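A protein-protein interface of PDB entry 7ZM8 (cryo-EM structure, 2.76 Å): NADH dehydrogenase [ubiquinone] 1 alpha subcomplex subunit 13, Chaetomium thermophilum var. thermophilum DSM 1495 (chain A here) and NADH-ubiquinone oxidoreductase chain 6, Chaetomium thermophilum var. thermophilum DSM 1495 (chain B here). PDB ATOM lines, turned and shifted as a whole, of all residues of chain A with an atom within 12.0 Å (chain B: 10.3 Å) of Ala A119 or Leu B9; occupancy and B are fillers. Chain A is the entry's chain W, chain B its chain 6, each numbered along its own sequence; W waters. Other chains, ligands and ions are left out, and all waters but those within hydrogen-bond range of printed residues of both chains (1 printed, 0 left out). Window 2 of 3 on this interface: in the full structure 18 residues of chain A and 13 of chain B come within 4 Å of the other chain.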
ATOM      1  N   ARG A  82      10.974  12.280  26.836  1.00  0.00           N
ATOM      2  CA  ARG A  82      10.122  12.383  25.628  1.00  0.00           C
ATOM      3  C   ARG A  82       8.773  11.729  25.848  1.00  0.00           C
ATOM      4  O   ARG A  82       7.809  12.180  25.240  1.00  0.00           O
ATOM      5  CB  ARG A  82      10.925  11.824  24.450  1.00  0.00           C
ATOM      6  CG  ARG A  82      12.243  12.559  24.256  1.00  0.00           C
ATOM      7  CD  ARG A  82      12.952  12.365  22.935  1.00  0.00           C
ATOM      8  NE  ARG A  82      12.108  12.647  21.789  1.00  0.00           N
ATOM      9  CZ  ARG A  82      12.567  12.996  20.599  1.00  0.00           C
ATOM     10  NH1 ARG A  82      11.728  13.232  19.609  1.00  0.00           N
ATOM     11  NH2 ARG A  82      13.863  13.129  20.407  1.00  0.00           N
ATOM     12  N   ARG A  89       1.500  16.183  25.466  1.00  0.00           N
ATOM     13  CA  ARG A  89       1.125  16.757  24.150  1.00  0.00           C
ATOM     14  C   ARG A  89      -0.227  16.184  23.750  1.00  0.00           C
ATOM     15  O   ARG A  89      -1.016  16.938  23.185  1.00  0.00           O
ATOM     16  CB  ARG A  89       2.222  16.407  23.145  1.00  0.00           C
ATOM     17  CG  ARG A  89       2.301  17.333  21.943  1.00  0.00           C
ATOM     18  CD  ARG A  89       3.544  17.089  21.114  1.00  0.00           C
ATOM     19  NE  ARG A  89       4.739  17.655  21.722  1.00  0.00           N
ATOM     20  CZ  ARG A  89       5.722  16.950  22.266  1.00  0.00           C
ATOM     21  NH1 ARG A  89       6.765  17.571  22.783  1.00  0.00           N
ATOM     22  NH2 ARG A  89       5.674  15.631  22.272  1.00  0.00           N
ATOM     23  N   PHE A 111       6.628   4.761  16.068  1.00  0.00           N
ATOM     24  CA  PHE A 111       6.283   5.938  15.247  1.00  0.00           C
ATOM     25  C   PHE A 111       6.288   7.144  16.175  1.00  0.00           C
ATOM     26  O   PHE A 111       6.184   6.962  17.383  1.00  0.00           O
ATOM     27  CB  PHE A 111       4.900   5.731  14.651  1.00  0.00           C
ATOM     28  CG  PHE A 111       4.679   4.450  13.898  1.00  0.00           C
ATOM     29  CD1 PHE A 111       5.128   4.311  12.599  1.00  0.00           C
ATOM     30  CD2 PHE A 111       3.970   3.409  14.469  1.00  0.00           C
ATOM     31  CE1 PHE A 111       4.886   3.146  11.895  1.00  0.00           C
ATOM     32  CE2 PHE A 111       3.750   2.237  13.770  1.00  0.00           C
ATOM     33  CZ  PHE A 111       4.209   2.108  12.484  1.00  0.00           C
ATOM     34  N   ALA A 112       6.445   8.336  15.620  1.00  0.00           N
ATOM     35  CA  ALA A 112       6.420   9.579  16.422  1.00  0.00           C
ATOM     36  C   ALA A 112       5.628  10.646  15.678  1.00  0.00           C
ATOM     37  O   ALA A 112       5.498  10.538  14.453  1.00  0.00           O
ATOM     38  CB  ALA A 112       7.822  10.065  16.621  1.00  0.00           C
ATOM     39  N   VAL A 113       5.126  11.650  16.384  1.00  0.00           N
ATOM     40  CA  VAL A 113       4.453  12.776  15.672  1.00  0.00           C
ATOM     41  C   VAL A 113       5.580  13.668  15.188  1.00  0.00           C
ATOM     42  O   VAL A 113       6.536  13.860  15.934  1.00  0.00           O
ATOM     43  CB  VAL A 113       3.426  13.529  16.536  1.00  0.00           C
ATOM     44  CG1 VAL A 113       2.955  14.815  15.897  1.00  0.00           C
ATOM     45  CG2 VAL A 113       2.259  12.641  16.919  1.00  0.00           C
ATOM     46  N   THR A 114       5.478  14.144  13.955  1.00  0.00           N
ATOM     47  CA  THR A 114       6.582  14.926  13.370  1.00  0.00           C
ATOM     48  C   THR A 114       6.039  16.271  12.921  1.00  0.00           C
ATOM     49  O   THR A 114       4.852  16.349  12.589  1.00  0.00           O
ATOM     50  CB  THR A 114       7.248  14.158  12.222  1.00  0.00           C
ATOM     51  OG1 THR A 114       6.221  13.666  11.365  1.00  0.00           O
ATOM     52  CG2 THR A 114       8.130  13.022  12.689  1.00  0.00           C
ATOM     53  N   PRO A 115       6.833  17.374  12.932  1.00  0.00           N
ATOM     54  CA  PRO A 115       6.356  18.624  12.371  1.00  0.00           C
ATOM     55  C   PRO A 115       6.088  18.423  10.877  1.00  0.00           C
ATOM     56  O   PRO A 115       6.710  17.577  10.278  1.00  0.00           O
ATOM     57  CB  PRO A 115       7.526  19.587  12.566  1.00  0.00           C
ATOM     58  CG  PRO A 115       8.254  19.038  13.757  1.00  0.00           C
ATOM     59  CD  PRO A 115       8.172  17.547  13.538  1.00  0.00           C
ATOM     60  N   SER A 116       5.190  19.221  10.309  1.00  0.00           N
ATOM     61  CA  SER A 116       4.825  19.089   8.877  1.00  0.00           C
ATOM     62  C   SER A 116       6.034  19.354   7.980  1.00  0.00           C
ATOM     63  O   SER A 116       6.137  18.687   6.943  1.00  0.00           O
ATOM     64  CB  SER A 116       3.675  19.994   8.553  1.00  0.00           C
ATOM     65  OG  SER A 116       3.853  21.265   9.158  1.00  0.00           O
ATOM     66  N   LYS A 117       6.890  20.312   8.345  1.00  0.00           N
ATOM     67  CA  LYS A 117       8.053  20.668   7.490  1.00  0.00           C
ATOM     68  C   LYS A 117       9.378  20.690   8.272  1.00  0.00           C
ATOM     69  O   LYS A 117       9.344  21.062   9.453  1.00  0.00           O
ATOM     70  CB  LYS A 117       7.857  22.048   6.855  1.00  0.00           C
ATOM     71  CG  LYS A 117       6.664  22.185   5.919  1.00  0.00           C
ATOM     72  CD  LYS A 117       6.758  21.309   4.688  1.00  0.00           C
ATOM     73  CE  LYS A 117       7.871  21.722   3.748  1.00  0.00           C
ATOM     74  NZ  LYS A 117       7.654  23.086   3.209  1.00  0.00           N
ATOM     75  N   PRO A 118      10.550  20.333   7.680  1.00  0.00           N
ATOM     76  CA  PRO A 118      11.822  20.475   8.375  1.00  0.00           C
ATOM     77  C   PRO A 118      12.295  21.928   8.517  1.00  0.00           C
ATOM     78  O   PRO A 118      11.758  22.784   7.840  1.00  0.00           O
ATOM     79  CB  PRO A 118      12.794  19.779   7.430  1.00  0.00           C
ATOM     80  CG  PRO A 118      11.932  18.897   6.568  1.00  0.00           C
ATOM     81  CD  PRO A 118      10.694  19.734   6.357  1.00  0.00           C
ATOM     82  N   ALA A 119      13.293  22.173   9.371  1.00  0.00           N
ATOM     83  CA  ALA A 119      13.856  23.535   9.554  1.00  0.00           C
ATOM     84  C   ALA A 119      14.374  24.079   8.217  1.00  0.00           C
ATOM     85  O   ALA A 119      15.037  23.312   7.497  1.00  0.00           O
ATOM     86  CB  ALA A 119      14.940  23.500  10.596  1.00  0.00           C
ATOM     87  N   GLN A 120      14.107  25.354   7.914  1.00  0.00           N
ATOM     88  CA  GLN A 120      14.479  25.953   6.599  1.00  0.00           C
ATOM     89  C   GLN A 120      15.890  25.580   6.135  1.00  0.00           C
ATOM     90  O   GLN A 120      16.012  25.203   4.953  1.00  0.00           O
ATOM     91  CB  GLN A 120      14.301  27.472   6.637  1.00  0.00           C
ATOM     92  CG  GLN A 120      12.877  27.930   6.353  1.00  0.00           C
ATOM     93  CD  GLN A 120      11.923  27.647   7.487  1.00  0.00           C
ATOM     94  OE1 GLN A 120      10.800  27.191   7.278  1.00  0.00           O
ATOM     95  NE2 GLN A 120      12.366  27.909   8.705  1.00  0.00           N
ATOM     96  N   GLU A 121      16.906  25.737   6.990  1.00  0.00           N
ATOM     97  CA  GLU A 121      18.293  25.448   6.624  1.00  0.00           C
ATOM     98  C   GLU A 121      18.787  26.369   5.511  1.00  0.00           C
ATOM     99  O   GLU A 121      18.366  27.520   5.411  1.00  0.00           O
ATOM    100  CB  GLU A 121      18.446  23.986   6.200  1.00  0.00           C
ATOM    101  N   ILE B   5       7.780  25.678  18.696  1.00  0.00           N
ATOM    102  CA  ILE B   5       7.458  24.224  18.606  1.00  0.00           C
ATOM    103  C   ILE B   5       8.488  23.416  19.396  1.00  0.00           C
ATOM    104  O   ILE B   5       9.699  23.615  19.197  1.00  0.00           O
ATOM    105  CB  ILE B   5       7.398  23.791  17.128  1.00  0.00           C
ATOM    106  CG1 ILE B   5       8.613  24.279  16.336  1.00  0.00           C
ATOM    107  CG2 ILE B   5       6.106  24.268  16.490  1.00  0.00           C
ATOM    108  CD1 ILE B   5       8.597  23.874  14.881  1.00  0.00           C
ATOM    109  N   SER B   6       8.009  22.567  20.305  1.00  0.00           N
ATOM    110  CA  SER B   6       8.922  21.684  21.069  1.00  0.00           C
ATOM    111  C   SER B   6       9.494  20.606  20.158  1.00  0.00           C
ATOM    112  O   SER B   6      10.679  20.291  20.300  1.00  0.00           O
ATOM    113  CB  SER B   6       8.243  21.118  22.266  1.00  0.00           C
ATOM    114  OG  SER B   6       8.042  22.124  23.245  1.00  0.00           O
ATOM    115  N   LEU B   7       8.671  20.060  19.266  1.00  0.00           N
ATOM    116  CA  LEU B   7       9.172  19.051  18.305  1.00  0.00           C
ATOM    117  C   LEU B   7       9.857  19.789  17.162  1.00  0.00           C
ATOM    118  O   LEU B   7       9.228  20.677  16.589  1.00  0.00           O
ATOM    119  CB  LEU B   7       8.014  18.186  17.799  1.00  0.00           C
ATOM    120  CG  LEU B   7       7.273  17.359  18.842  1.00  0.00           C
ATOM    121  CD1 LEU B   7       6.064  16.692  18.208  1.00  0.00           C
ATOM    122  CD2 LEU B   7       8.192  16.321  19.464  1.00  0.00           C
ATOM    123  N   LEU B   8      11.111  19.436  16.868  1.00  0.00           N
ATOM    124  CA  LEU B   8      11.891  20.103  15.793  1.00  0.00           C
ATOM    125  C   LEU B   8      12.399  19.059  14.792  1.00  0.00           C
ATOM    126  O   LEU B   8      12.994  18.071  15.236  1.00  0.00           O
ATOM    127  CB  LEU B   8      13.064  20.845  16.438  1.00  0.00           C
ATOM    128  CG  LEU B   8      12.697  21.989  17.378  1.00  0.00           C
ATOM    129  CD1 LEU B   8      13.907  22.421  18.186  1.00  0.00           C
ATOM    130  CD2 LEU B   8      12.136  23.164  16.598  1.00  0.00           C
ATOM    131  N   LEU B   9      12.222  19.306  13.490  1.00  0.00           N
ATOM    132  CA  LEU B   9      12.655  18.349  12.435  1.00  0.00           C
ATOM    133  C   LEU B   9      13.857  18.926  11.677  1.00  0.00           C
ATOM    134  O   LEU B   9      13.751  20.068  11.217  1.00  0.00           O
ATOM    135  CB  LEU B   9      11.467  18.079  11.508  1.00  0.00           C
ATOM    136  CG  LEU B   9      11.498  16.748  10.760  1.00  0.00           C
ATOM    137  CD1 LEU B   9      11.683  15.588  11.726  1.00  0.00           C
ATOM    138  CD2 LEU B   9      10.226  16.565   9.950  1.00  0.00           C
ATOM    139  N   LEU B  10      14.954  18.171  11.568  1.00  0.00           N
ATOM    140  CA  LEU B  10      16.199  18.662  10.912  1.00  0.00           C
ATOM    141  C   LEU B  10      16.715  17.602   9.936  1.00  0.00           C
ATOM    142  O   LEU B  10      16.373  16.432  10.122  1.00  0.00           O
ATOM    143  CB  LEU B  10      17.271  18.880  11.982  1.00  0.00           C
ATOM    144  CG  LEU B  10      17.173  20.146  12.821  1.00  0.00           C
ATOM    145  CD1 LEU B  10      16.547  19.837  14.174  1.00  0.00           C
ATOM    146  CD2 LEU B  10      18.561  20.735  13.006  1.00  0.00           C
ATOM    147  N   LYS B  11      17.518  17.996   8.946  1.00  0.00           N
ATOM    148  CA  LYS B  11      18.134  17.007   8.023  1.00  0.00           C
ATOM    149  C   LYS B  11      19.473  16.537   8.596  1.00  0.00           C
ATOM    150  O   LYS B  11      20.276  17.400   8.966  1.00  0.00           O
ATOM    151  CB  LYS B  11      18.355  17.607   6.635  1.00  0.00           C
ATOM    152  CG  LYS B  11      18.715  16.606   5.547  1.00  0.00           C
ATOM    153  CD  LYS B  11      18.802  17.221   4.168  1.00  0.00           C
ATOM    154  CE  LYS B  11      19.062  16.199   3.082  1.00  0.00           C
ATOM    155  NZ  LYS B  11      19.087  16.821   1.737  1.00  0.00           N
ATOM    156  N   GLU B  12      19.688  15.216   8.681  1.00  0.00           N
ATOM    157  CA  GLU B  12      20.997  14.675   9.131  1.00  0.00           C
ATOM    158  C   GLU B  12      22.085  15.019   8.110  1.00  0.00           C
ATOM    159  O   GLU B  12      21.755  15.125   6.919  1.00  0.00           O
ATOM    160  CB  GLU B  12      20.891  13.168   9.338  1.00  0.00           C
ATOM    161  CG  GLU B  12      19.617  12.758  10.040  1.00  0.00           C
ATOM    162  CD  GLU B  12      19.461  11.257  10.176  1.00  0.00           C
ATOM    163  OE1 GLU B  12      18.377  10.808  10.581  1.00  0.00           O
ATOM    164  OE2 GLU B  12      20.431  10.548   9.881  1.00  0.00           O
ATOM    165  N   ASP B 166       1.624  11.612   7.330  1.00  0.00           N
ATOM    166  CA  ASP B 166       2.179  10.284   7.132  1.00  0.00           C
ATOM    167  C   ASP B 166       2.963   9.873   8.365  1.00  0.00           C
ATOM    168  O   ASP B 166       3.593  10.707   9.020  1.00  0.00           O
ATOM    169  CB  ASP B 166       3.083  10.235   5.895  1.00  0.00           C
ATOM    170  CG  ASP B 166       2.989   8.915   5.161  1.00  0.00           C
ATOM    171  OD1 ASP B 166       2.722   7.887   5.815  1.00  0.00           O
ATOM    172  OD2 ASP B 166       3.182   8.905   3.927  1.00  0.00           O
ATOM    173  N   LEU B 167       2.909   8.586   8.682  1.00  0.00           N
ATOM    174  CA  LEU B 167       3.684   8.051   9.785  1.00  0.00           C
ATOM    175  C   LEU B 167       5.166   8.072   9.455  1.00  0.00           C
ATOM    176  O   LEU B 167       5.571   7.896   8.306  1.00  0.00           O
ATOM    177  CB  LEU B 167       3.259   6.622  10.090  1.00  0.00           C
ATOM    178  CG  LEU B 167       2.001   6.414  10.914  1.00  0.00           C
ATOM    179  CD1 LEU B 167       1.668   4.950  10.921  1.00  0.00           C
ATOM    180  CD2 LEU B 167       2.219   6.921  12.313  1.00  0.00           C
ATOM    181  N   PHE B 168       5.976   8.303  10.482  1.00  0.00           N
ATOM    182  CA  PHE B 168       7.438   8.188  10.287  1.00  0.00           C
ATOM    183  C   PHE B 168       7.906   7.162  11.315  1.00  0.00           C
ATOM    184  O   PHE B 168       7.309   7.105  12.386  1.00  0.00           O
ATOM    185  CB  PHE B 168       8.121   9.542  10.483  1.00  0.00           C
ATOM    186  CG  PHE B 168       8.163  10.432   9.267  1.00  0.00           C
ATOM    187  CD1 PHE B 168       7.087  11.236   8.935  1.00  0.00           C
ATOM    188  CD2 PHE B 168       9.290  10.480   8.465  1.00  0.00           C
ATOM    189  CE1 PHE B 168       7.130  12.059   7.821  1.00  0.00           C
ATOM    190  CE2 PHE B 168       9.334  11.302   7.350  1.00  0.00           C
ATOM    191  CZ  PHE B 168       8.254  12.090   7.031  1.00  0.00           C
ATOM    192  N   PHE B 169       8.959   6.409  11.002  1.00  0.00           N
ATOM    193  CA  PHE B 169       9.493   5.383  11.932  1.00  0.00           C
ATOM    194  C   PHE B 169      10.615   6.011  12.753  1.00  0.00           C
ATOM    195  O   PHE B 169      11.632   6.395  12.175  1.00  0.00           O
ATOM    196  CB  PHE B 169      10.026   4.184  11.148  1.00  0.00           C
ATOM    197  CG  PHE B 169       8.975   3.234  10.646  1.00  0.00           C
ATOM    198  CD1 PHE B 169       8.522   2.199  11.445  1.00  0.00           C
ATOM    199  CD2 PHE B 169       8.447   3.371   9.374  1.00  0.00           C
ATOM    200  CE1 PHE B 169       7.557   1.320  10.982  1.00  0.00           C
ATOM    201  CE2 PHE B 169       7.482   2.493   8.913  1.00  0.00           C
ATOM    202  CZ  PHE B 169       7.041   1.469   9.718  1.00  0.00           C
ATOM    203  N   ILE B 170      10.421   6.109  14.064  1.00  0.00           N
ATOM    204  CA  ILE B 170      11.437   6.733  14.961  1.00  0.00           C
ATOM    205  C   ILE B 170      12.403   5.668  15.484  1.00  0.00           C
ATOM    206  O   ILE B 170      11.960   4.546  15.743  1.00  0.00           O
ATOM    207  CB  ILE B 170      10.780   7.566  16.086  1.00  0.00           C
ATOM    208  CG1 ILE B 170      11.774   8.509  16.769  1.00  0.00           C
ATOM    209  CG2 ILE B 170      10.037   6.696  17.085  1.00  0.00           C
ATOM    210  CD1 ILE B 170      11.947   9.824  16.058  1.00  0.00           C
HETATM  211  O   HOH W   1       5.224  11.089  11.618  1.00  0.00           O
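N of Ala A119 lies within hydrogen-bond range of O of Leu B9 (2.8 Å).
Among the printed residues, merely in contact across the chains: Phe A111 with Phe B168, Phe A111 with Phe B169, Pro A115 with Leu B7, Pro A118 with Leu B9, Thr A114 with Phe B168, Ala A112 with Phe B168, Val A113 with Leu B7, Pro A115 with Leu B9, Phe A111 with Leu B167, Arg A89 with Leu B7, Phe A111 with Ile B170, Arg A89 with Ser B6 and Ala A112 with Ile B170.
Of the printed residues of chain B, Ala A119 touches Leu B9 (2.8 Å).
Leu B9 touches just these residues of chain A: Pro A115, Pro A118 and Ala A119.
Of chain B, only Leu B7 (3.4 Å) and Leu B9 (3.7 Å) come within 4 Å of Pro A115.
No residue of chain B comes within 4 Å of Gln A120.
No residue of chain B comes within 4 Å of Glu A121.
No residue of chain A comes within 4 Å of Leu B10.
Of the printed residues of chain A, Ser B6 touches Arg A89 (3.9 Å).
Of the printed residues of chain A, Phe B169 touches Phe A111 (3.4 Å).
Lys A117 touches none of the printed residues of chain B.
Lys B11 touches none of the printed residues of chain A.
The nearest residue of chain B that does not touch Ala A119 is Leu B10 (4.6 Å).
The nearest printed residue of chain B that does not touch Phe A111 is Asp B166 (7.3 Å).
Of the 13 printed residues of chain A, 8 touch a printed residue of chain B.
Among the printed residues, 14 pairs touch across the chains.
Among the printed residues, no Asp or Glu carboxylate lies within 4 Å of a Lys or Arg side-chain nitrogen of the other chain.
Water W1 lies within hydrogen-bond range of the side-chain hydroxyl (OG1) of Thr A114, the backbone carbonyl oxygen (O) of Ala A112, the backbone carbonyl oxygen (O) of Asp B166 and the backbone NH (N) of Phe B168.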
